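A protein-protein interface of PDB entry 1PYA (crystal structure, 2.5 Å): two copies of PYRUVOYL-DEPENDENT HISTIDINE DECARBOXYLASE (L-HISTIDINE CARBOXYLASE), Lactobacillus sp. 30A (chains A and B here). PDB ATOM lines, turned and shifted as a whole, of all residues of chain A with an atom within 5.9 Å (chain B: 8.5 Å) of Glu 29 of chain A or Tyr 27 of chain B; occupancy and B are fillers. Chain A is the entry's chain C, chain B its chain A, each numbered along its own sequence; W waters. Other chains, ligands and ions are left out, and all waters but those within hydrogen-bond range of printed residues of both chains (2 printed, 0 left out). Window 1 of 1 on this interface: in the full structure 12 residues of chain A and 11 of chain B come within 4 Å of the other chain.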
ATOM      1  N   THR A  24       8.816  13.703 -24.083  1.00  0.00           N
ATOM      2  CA  THR A  24       8.171  13.809 -25.394  1.00  0.00           C
ATOM      3  C   THR A  24       6.752  14.399 -25.138  1.00  0.00           C
ATOM      4  O   THR A  24       6.260  14.497 -23.986  1.00  0.00           O
ATOM      5  CB  THR A  24       7.998  12.427 -26.082  1.00  0.00           C
ATOM      6  OG1 THR A  24       7.659  11.511 -25.056  1.00  0.00           O
ATOM      7  CG2 THR A  24       9.221  11.964 -26.795  1.00  0.00           C
ATOM      8  N   ARG A  25       6.081  14.799 -26.199  1.00  0.00           N
ATOM      9  CA  ARG A  25       4.717  15.292 -26.094  1.00  0.00           C
ATOM     10  C   ARG A  25       3.974  14.699 -27.298  1.00  0.00           C
ATOM     11  O   ARG A  25       4.595  14.123 -28.201  1.00  0.00           O
ATOM     12  CB  ARG A  25       4.656  16.826 -26.167  1.00  0.00           C
ATOM     13  CG  ARG A  25       5.378  17.555 -25.048  1.00  0.00           C
ATOM     14  CD  ARG A  25       5.285  19.041 -25.291  1.00  0.00           C
ATOM     15  NE  ARG A  25       4.002  19.568 -24.829  1.00  0.00           N
ATOM     16  CZ  ARG A  25       3.373  20.568 -25.469  1.00  0.00           C
ATOM     17  NH1 ARG A  25       3.821  21.055 -26.637  1.00  0.00           N
ATOM     18  NH2 ARG A  25       2.256  21.057 -24.957  1.00  0.00           N
ATOM     19  N   GLY A  26       2.663  14.806 -27.359  1.00  0.00           N
ATOM     20  CA  GLY A  26       1.916  14.251 -28.461  1.00  0.00           C
ATOM     21  C   GLY A  26       1.687  15.250 -29.575  1.00  0.00           C
ATOM     22  O   GLY A  26       1.716  16.482 -29.392  1.00  0.00           O
ATOM     23  N   TYR A  27       1.522  14.648 -30.742  1.00  0.00           N
ATOM     24  CA  TYR A  27       1.124  15.334 -31.958  1.00  0.00           C
ATOM     25  C   TYR A  27      -0.190  16.104 -31.702  1.00  0.00           C
ATOM     26  O   TYR A  27      -1.146  15.577 -31.107  1.00  0.00           O
ATOM     27  CB  TYR A  27       0.949  14.271 -33.034  1.00  0.00           C
ATOM     28  CG  TYR A  27       0.466  14.821 -34.361  1.00  0.00           C
ATOM     29  CD1 TYR A  27       1.251  15.702 -35.066  1.00  0.00           C
ATOM     30  CD2 TYR A  27      -0.758  14.448 -34.855  1.00  0.00           C
ATOM     31  CE1 TYR A  27       0.816  16.206 -36.267  1.00  0.00           C
ATOM     32  CE2 TYR A  27      -1.196  14.964 -36.056  1.00  0.00           C
ATOM     33  CZ  TYR A  27      -0.410  15.841 -36.741  1.00  0.00           C
ATOM     34  OH  TYR A  27      -0.870  16.388 -37.908  1.00  0.00           O
ATOM     35  N   MET A  28      -0.273  17.326 -32.246  1.00  0.00           N
ATOM     36  CA  MET A  28      -1.330  18.345 -32.119  1.00  0.00           C
ATOM     37  C   MET A  28      -1.304  19.095 -30.791  1.00  0.00           C
ATOM     38  O   MET A  28      -2.115  20.004 -30.577  1.00  0.00           O
ATOM     39  CB  MET A  28      -2.755  17.807 -32.268  1.00  0.00           C
ATOM     40  CG  MET A  28      -2.907  17.236 -33.677  1.00  0.00           C
ATOM     41  SD  MET A  28      -4.512  16.484 -34.082  1.00  0.00           S
ATOM     42  CE  MET A  28      -4.199  14.825 -33.580  1.00  0.00           C
ATOM     43  N   GLU A  29      -0.434  18.808 -29.835  1.00  0.00           N
ATOM     44  CA  GLU A  29      -0.417  19.598 -28.605  1.00  0.00           C
ATOM     45  C   GLU A  29       0.144  21.000 -28.841  1.00  0.00           C
ATOM     46  O   GLU A  29       1.091  21.128 -29.633  1.00  0.00           O
ATOM     47  CB  GLU A  29       0.384  18.867 -27.559  1.00  0.00           C
ATOM     48  CG  GLU A  29      -0.354  17.637 -27.076  1.00  0.00           C
ATOM     49  CD  GLU A  29       0.140  17.206 -25.720  1.00  0.00           C
ATOM     50  OE1 GLU A  29       1.235  16.667 -25.638  1.00  0.00           O
ATOM     51  OE2 GLU A  29      -0.548  17.428 -24.732  1.00  0.00           O
ATOM     52  N   PRO A  30      -0.410  22.069 -28.246  1.00  0.00           N
ATOM     53  CA  PRO A  30       0.023  23.463 -28.440  1.00  0.00           C
ATOM     54  C   PRO A  30       1.457  23.678 -28.052  1.00  0.00           C
ATOM     55  O   PRO A  30       1.823  23.202 -26.977  1.00  0.00           O
ATOM     56  CB  PRO A  30      -0.879  24.292 -27.583  1.00  0.00           C
ATOM     57  CG  PRO A  30      -1.395  23.302 -26.553  1.00  0.00           C
ATOM     58  CD  PRO A  30      -1.553  22.002 -27.336  1.00  0.00           C
ATOM     59  N   GLY A  31       2.294  24.354 -28.876  1.00  0.00           N
ATOM     60  CA  GLY A  31       3.683  24.573 -28.503  1.00  0.00           C
ATOM     61  C   GLY A  31       4.715  23.670 -29.159  1.00  0.00           C
ATOM     62  O   GLY A  31       5.903  23.910 -28.987  1.00  0.00           O
ATOM     63  N   ASN A  32       4.358  22.593 -29.829  1.00  0.00           N
ATOM     64  CA  ASN A  32       5.326  21.778 -30.558  1.00  0.00           C
ATOM     65  C   ASN A  32       5.824  22.540 -31.761  1.00  0.00           C
ATOM     66  O   ASN A  32       5.090  23.377 -32.284  1.00  0.00           O
ATOM     67  CB  ASN A  32       4.726  20.477 -31.073  1.00  0.00           C
ATOM     68  CG  ASN A  32       4.407  19.505 -29.960  1.00  0.00           C
ATOM     69  OD1 ASN A  32       4.930  19.601 -28.853  1.00  0.00           O
ATOM     70  ND2 ASN A  32       3.566  18.504 -30.192  1.00  0.00           N
ATOM     71  N   ASP B  13       4.237  25.540 -19.410  1.00  0.00           N
ATOM     72  CA  ASP B  13       3.451  26.617 -18.848  1.00  0.00           C
ATOM     73  C   ASP B  13       2.059  26.027 -18.762  1.00  0.00           C
ATOM     74  O   ASP B  13       1.691  25.060 -19.454  1.00  0.00           O
ATOM     75  CB  ASP B  13       3.415  27.885 -19.741  1.00  0.00           C
ATOM     76  CG  ASP B  13       2.750  27.799 -21.092  1.00  0.00           C
ATOM     77  OD1 ASP B  13       1.520  27.795 -21.164  1.00  0.00           O
ATOM     78  OD2 ASP B  13       3.478  27.739 -22.081  1.00  0.00           O
ATOM     79  N   ILE B  15      -0.748  28.171 -19.133  1.00  0.00           N
ATOM     80  CA  ILE B  15      -1.630  29.222 -19.642  1.00  0.00           C
ATOM     81  C   ILE B  15      -2.637  28.579 -20.576  1.00  0.00           C
ATOM     82  O   ILE B  15      -2.241  27.793 -21.462  1.00  0.00           O
ATOM     83  CB  ILE B  15      -0.752  30.331 -20.383  1.00  0.00           C
ATOM     84  CG1 ILE B  15       0.097  31.037 -19.331  1.00  0.00           C
ATOM     85  CG2 ILE B  15      -1.637  31.338 -21.166  1.00  0.00           C
ATOM     86  CD1 ILE B  15       1.388  31.583 -19.929  1.00  0.00           C
ATOM     87  N   ALA B  16      -3.894  28.920 -20.397  1.00  0.00           N
ATOM     88  CA  ALA B  16      -4.956  28.362 -21.193  1.00  0.00           C
ATOM     89  C   ALA B  16      -5.990  29.471 -21.420  1.00  0.00           C
ATOM     90  O   ALA B  16      -6.953  29.586 -20.653  1.00  0.00           O
ATOM     91  CB  ALA B  16      -5.592  27.196 -20.429  1.00  0.00           C
ATOM     92  N   THR B  24     -15.717  29.110 -23.280  1.00  0.00           N
ATOM     93  CA  THR B  24     -14.499  28.373 -23.083  1.00  0.00           C
ATOM     94  C   THR B  24     -14.376  27.572 -24.384  1.00  0.00           C
ATOM     95  O   THR B  24     -15.294  27.468 -25.235  1.00  0.00           O
ATOM     96  CB  THR B  24     -14.550  27.386 -21.888  1.00  0.00           C
ATOM     97  OG1 THR B  24     -15.830  26.788 -21.851  1.00  0.00           O
ATOM     98  CG2 THR B  24     -14.345  28.072 -20.557  1.00  0.00           C
ATOM     99  N   ARG B  25     -13.197  26.993 -24.545  1.00  0.00           N
ATOM    100  CA  ARG B  25     -12.803  26.227 -25.732  1.00  0.00           C
ATOM    101  C   ARG B  25     -11.994  25.024 -25.265  1.00  0.00           C
ATOM    102  O   ARG B  25     -11.561  24.996 -24.095  1.00  0.00           O
ATOM    103  CB  ARG B  25     -11.938  27.094 -26.649  1.00  0.00           C
ATOM    104  CG  ARG B  25     -12.843  27.681 -27.711  1.00  0.00           C
ATOM    105  CD  ARG B  25     -12.295  28.837 -28.503  1.00  0.00           C
ATOM    106  NE  ARG B  25     -10.917  28.795 -28.925  1.00  0.00           N
ATOM    107  CZ  ARG B  25     -10.408  28.378 -30.092  1.00  0.00           C
ATOM    108  NH1 ARG B  25     -11.069  27.843 -31.117  1.00  0.00           N
ATOM    109  NH2 ARG B  25      -9.094  28.550 -30.157  1.00  0.00           N
ATOM    110  N   GLY B  26     -11.749  24.054 -26.122  1.00  0.00           N
ATOM    111  CA  GLY B  26     -11.017  22.889 -25.712  1.00  0.00           C
ATOM    112  C   GLY B  26      -9.531  23.063 -25.849  1.00  0.00           C
ATOM    113  O   GLY B  26      -9.010  23.838 -26.675  1.00  0.00           O
ATOM    114  N   TYR B  27      -8.844  22.287 -25.006  1.00  0.00           N
ATOM    115  CA  TYR B  27      -7.399  22.147 -25.110  1.00  0.00           C
ATOM    116  C   TYR B  27      -7.055  21.616 -26.524  1.00  0.00           C
ATOM    117  O   TYR B  27      -7.655  20.628 -26.987  1.00  0.00           O
ATOM    118  CB  TYR B  27      -6.955  21.176 -24.013  1.00  0.00           C
ATOM    119  CG  TYR B  27      -5.491  20.792 -24.109  1.00  0.00           C
ATOM    120  CD1 TYR B  27      -4.531  21.782 -24.024  1.00  0.00           C
ATOM    121  CD2 TYR B  27      -5.138  19.474 -24.321  1.00  0.00           C
ATOM    122  CE1 TYR B  27      -3.199  21.462 -24.156  1.00  0.00           C
ATOM    123  CE2 TYR B  27      -3.805  19.151 -24.450  1.00  0.00           C
ATOM    124  CZ  TYR B  27      -2.850  20.147 -24.380  1.00  0.00           C
ATOM    125  OH  TYR B  27      -1.518  19.826 -24.531  1.00  0.00           O
ATOM    126  N   MET B  28      -6.073  22.227 -27.215  1.00  0.00           N
ATOM    127  CA  MET B  28      -5.590  21.935 -28.563  1.00  0.00           C
ATOM    128  C   MET B  28      -6.400  22.577 -29.698  1.00  0.00           C
ATOM    129  O   MET B  28      -6.031  22.435 -30.869  1.00  0.00           O
ATOM    130  CB  MET B  28      -5.541  20.428 -28.886  1.00  0.00           C
ATOM    131  CG  MET B  28      -4.565  19.624 -27.997  1.00  0.00           C
ATOM    132  SD  MET B  28      -4.450  17.818 -28.274  1.00  0.00           S
ATOM    133  CE  MET B  28      -5.948  17.330 -27.489  1.00  0.00           C
ATOM    134  N   GLU B  29      -7.490  23.308 -29.464  1.00  0.00           N
ATOM    135  CA  GLU B  29      -8.199  23.979 -30.559  1.00  0.00           C
ATOM    136  C   GLU B  29      -7.381  25.186 -30.973  1.00  0.00           C
ATOM    137  O   GLU B  29      -6.840  25.900 -30.094  1.00  0.00           O
ATOM    138  CB  GLU B  29      -9.578  24.479 -30.148  1.00  0.00           C
ATOM    139  CG  GLU B  29     -10.447  23.316 -29.732  1.00  0.00           C
ATOM    140  CD  GLU B  29     -11.914  23.629 -29.823  1.00  0.00           C
ATOM    141  OE1 GLU B  29     -12.408  24.296 -28.929  1.00  0.00           O
ATOM    142  OE2 GLU B  29     -12.547  23.222 -30.790  1.00  0.00           O
ATOM    143  N   PRO B  30      -7.261  25.426 -32.278  1.00  0.00           N
ATOM    144  CA  PRO B  30      -6.339  26.398 -32.827  1.00  0.00           C
ATOM    145  C   PRO B  30      -6.804  27.765 -32.402  1.00  0.00           C
ATOM    146  O   PRO B  30      -8.003  28.035 -32.453  1.00  0.00           O
ATOM    147  CB  PRO B  30      -6.386  26.176 -34.325  1.00  0.00           C
ATOM    148  CG  PRO B  30      -7.784  25.728 -34.580  1.00  0.00           C
ATOM    149  CD  PRO B  30      -8.015  24.781 -33.369  1.00  0.00           C
ATOM    150  N   ASN B  32      -6.057  29.186 -29.265  1.00  0.00           N
ATOM    151  CA  ASN B  32      -5.929  29.431 -27.822  1.00  0.00           C
ATOM    152  C   ASN B  32      -4.555  30.009 -27.524  1.00  0.00           C
ATOM    153  O   ASN B  32      -3.588  29.800 -28.287  1.00  0.00           O
ATOM    154  CB  ASN B  32      -6.087  28.139 -27.017  1.00  0.00           C
ATOM    155  CG  ASN B  32      -7.507  27.577 -27.102  1.00  0.00           C
ATOM    156  OD1 ASN B  32      -8.481  28.269 -27.421  1.00  0.00           O
ATOM    157  ND2 ASN B  32      -7.659  26.292 -26.806  1.00  0.00           N
ATOM    158  N   GLY B  34      -1.364  30.141 -24.940  1.00  0.00           N
ATOM    159  CA  GLY B  34      -0.734  29.289 -23.940  1.00  0.00           C
ATOM    160  C   GLY B  34      -0.766  27.807 -24.318  1.00  0.00           C
ATOM    161  O   GLY B  34      -1.531  27.387 -25.185  1.00  0.00           O
ATOM    162  N   ASN B  35       0.050  27.008 -23.630  1.00  0.00           N
ATOM    163  CA  ASN B  35       0.158  25.572 -23.882  1.00  0.00           C
ATOM    164  C   ASN B  35      -0.307  24.713 -22.706  1.00  0.00           C
ATOM    165  O   ASN B  35       0.072  23.549 -22.580  1.00  0.00           O
ATOM    166  CB  ASN B  35       1.588  25.214 -24.193  1.00  0.00           C
ATOM    167  CG  ASN B  35       2.190  26.043 -25.319  1.00  0.00           C
ATOM    168  OD1 ASN B  35       1.514  26.385 -26.270  1.00  0.00           O
ATOM    169  ND2 ASN B  35       3.474  26.368 -25.329  1.00  0.00           N
ATOM    170  N   GLY B  36      -1.112  25.281 -21.803  1.00  0.00           N
ATOM    171  CA  GLY B  36      -1.664  24.569 -20.670  1.00  0.00           C
ATOM    172  C   GLY B  36      -3.150  24.274 -20.862  1.00  0.00           C
ATOM    173  O   GLY B  36      -3.693  24.402 -21.971  1.00  0.00           O
ATOM    174  N   TYR B  37      -3.805  23.878 -19.773  1.00  0.00           N
ATOM    175  CA  TYR B  37      -5.207  23.549 -19.800  1.00  0.00           C
ATOM    176  C   TYR B  37      -5.771  23.623 -18.387  1.00  0.00           C
ATOM    177  O   TYR B  37      -5.047  23.574 -17.364  1.00  0.00           O
ATOM    178  CB  TYR B  37      -5.429  22.121 -20.379  1.00  0.00           C
ATOM    179  CG  TYR B  37      -4.675  20.929 -19.781  1.00  0.00           C
ATOM    180  CD1 TYR B  37      -5.014  20.451 -18.522  1.00  0.00           C
ATOM    181  CD2 TYR B  37      -3.704  20.280 -20.523  1.00  0.00           C
ATOM    182  CE1 TYR B  37      -4.388  19.330 -17.985  1.00  0.00           C
ATOM    183  CE2 TYR B  37      -3.081  19.156 -19.979  1.00  0.00           C
ATOM    184  CZ  TYR B  37      -3.423  18.685 -18.714  1.00  0.00           C
ATOM    185  OH  TYR B  37      -2.747  17.628 -18.115  1.00  0.00           O
ATOM    186  N   VAL B  38      -7.101  23.705 -18.348  1.00  0.00           N
ATOM    187  CA  VAL B  38      -7.807  23.778 -17.085  1.00  0.00           C
ATOM    188  C   VAL B  38      -8.854  22.664 -17.146  1.00  0.00           C
ATOM    189  O   VAL B  38      -9.391  22.371 -18.235  1.00  0.00           O
ATOM    190  CB  VAL B  38      -8.472  25.173 -16.923  1.00  0.00           C
ATOM    191  CG1 VAL B  38      -9.269  25.214 -15.629  1.00  0.00           C
ATOM    192  CG2 VAL B  38      -7.441  26.286 -16.794  1.00  0.00           C
ATOM    193  N   THR B  39      -9.176  22.012 -16.031  1.00  0.00           N
ATOM    194  CA  THR B  39     -10.146  20.944 -16.033  1.00  0.00           C
ATOM    195  C   THR B  39     -11.076  21.155 -14.833  1.00  0.00           C
ATOM    196  O   THR B  39     -10.907  22.103 -14.047  1.00  0.00           O
ATOM    197  CB  THR B  39      -9.299  19.620 -16.008  1.00  0.00           C
ATOM    198  OG1 THR B  39     -10.213  18.582 -16.274  1.00  0.00           O
ATOM    199  CG2 THR B  39      -8.559  19.351 -14.721  1.00  0.00           C
ATOM    200  N   THR B  78     -14.410  14.443 -27.401  1.00  0.00           N
ATOM    201  CA  THR B  78     -13.347  13.521 -27.757  1.00  0.00           C
ATOM    202  C   THR B  78     -12.964  12.765 -26.490  1.00  0.00           C
ATOM    203  O   THR B  78     -13.043  13.364 -25.401  1.00  0.00           O
ATOM    204  CB  THR B  78     -12.268  14.435 -28.328  1.00  0.00           C
ATOM    205  OG1 THR B  78     -12.612  14.474 -29.724  1.00  0.00           O
ATOM    206  CG2 THR B  78     -10.837  14.008 -28.105  1.00  0.00           C
HETATM  207  O   HOH W   1       1.834  27.756 -28.891  1.00  0.00           O
HETATM  208  O   HOH W   2      -3.016  22.019 -32.103  1.00  0.00           O
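The backbone NH of Gly 31 of chain A lies within hydrogen-bond range of the side-chain amide oxygen of Asn 35 of chain B (3.4 Å).
OD1 of Asn 35 of chain B sits close to O of Pro 30 of chain A (3.3 Å).
The side-chain hydroxyl of Tyr 27 of chain B lies within hydrogen-bond range of the side-chain carboxylate of Glu 29 of chain A, 2.6 Å away.
Printed residues of chain B that touch a printed residue of chain A: Tyr 27, Met 28, Gly 34 and Asn 35.
Hydrophobic or aromatic side chains of chain A that line the printed part of chain B: Pro 30.
Among the printed residues, no Asp or Glu carboxylate lies within 4 Å of a Lys or Arg side-chain nitrogen of the other chain.
Glu 29 of chain A touches just one residue of chain B: Tyr 27 (2.6 Å).
Of the printed residues of chain A, Tyr 27 of chain B touches Arg 25, Glu 29 and Pro 30.
Pro 30 of chain A touches just these residues of chain B: Tyr 27 (3.5 Å), Met 28 (3.9 Å), Gly 34 (3.97 Å) and Asn 35 (3.2 Å).
Printed residues of chain A within 4 Å of Met 28 of chain B: Met 28 (3.6 Å) and Pro 30 (3.9 Å).
Of the printed residues of chain B, Arg 25 of chain A touches Tyr 27.
Of the printed residues of chain A, Asn 35 of chain B touches Pro 30 and Gly 31.
Printed residues of chain A within 4 Å of Gly 34 of chain B: Pro 30 (3.97 Å).
Pro 30 of chain B touches none of the printed residues of chain A.
Arg 25 of chain B touches none of the printed residues of chain A.
The nearest residue of chain B that does not touch Glu 29 of chain A is Met 28 of chain B (4.2 Å).
The nearest printed residue of chain A that does not touch Tyr 27 of chain B is Met 28 of chain A (6.1 Å).
The nearest printed residue of chain A that does not touch Asn 35 of chain B is Arg 25 of chain A (4.1 Å).
Water W2 lies within hydrogen-bond range of the backbone carbonyl oxygen (O) of Met 28 of chain A (2.7 Å) and the backbone carbonyl oxygen (O) of Met 28 of chain B (3.3 Å).
Water W1 lies within hydrogen-bond range of the side-chain amide oxygen of Asn 35 of chain B (3.0 Å) and the backbone NH of Gly 31 of chain A (3.4 Å).
Met 28 of chain B touches its own counterpart, Met 28 of chain A.
Glu 29 of chain A touches Tyr 27 of chain B, but with the chains exchanged Tyr 27 of chain A does not touch Glu 29 of chain B (10.1 Å).
Pro 30 of chain A touches Tyr 27 of chain B, but with the chains exchanged Tyr 27 of chain A does not touch Pro 30 of chain B (11.7 Å).
Pro 30 of chain A touches Met 28 of chain B, but with the chains exchanged Met 28 of chain A does not touch Pro 30 of chain B (7.7 Å).
Of the 8 pairs that touch across the chains among the printed residues, 1 has its exchanged pair printed and touching as well.
OD1 of Asp 13 of chain B lies within hydrogen-bond range of N of Asn 35 of chain B, 3.0 Å away.
The side-chain amide oxygen of Asn 32 of chain A is in hydrogen-bond range of the guanidinium group of Arg 25 of chain A, at 2.9 Å.
OE1 of Glu 29 of chain A lies within hydrogen-bond range of N of Gly 26 of chain A (2.9 Å).
The backbone NH (N) of Asn 35 of chain B sits at hydrogen-bond distance from the backbone carbonyl oxygen (O) of Ile 15 of chain B, 3.3 Å away.
NH1 of Arg 25 of chain A sits at hydrogen-bond distance from O of Pro 30 of chain A (3.0 Å).
Tyr 27 of chain B touches Arg 25 of chain A (OH to NH2, 3.99 Å).
Met 28 of chain B touches Met 28 of chain A.
Pro 30 of chain A touches Tyr 27 of chain B (CG to CE1, 3.5 Å).
Met 28 of chain B touches Pro 30 of chain A.
Pro 30 of chain A touches Gly 34 of chain B.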
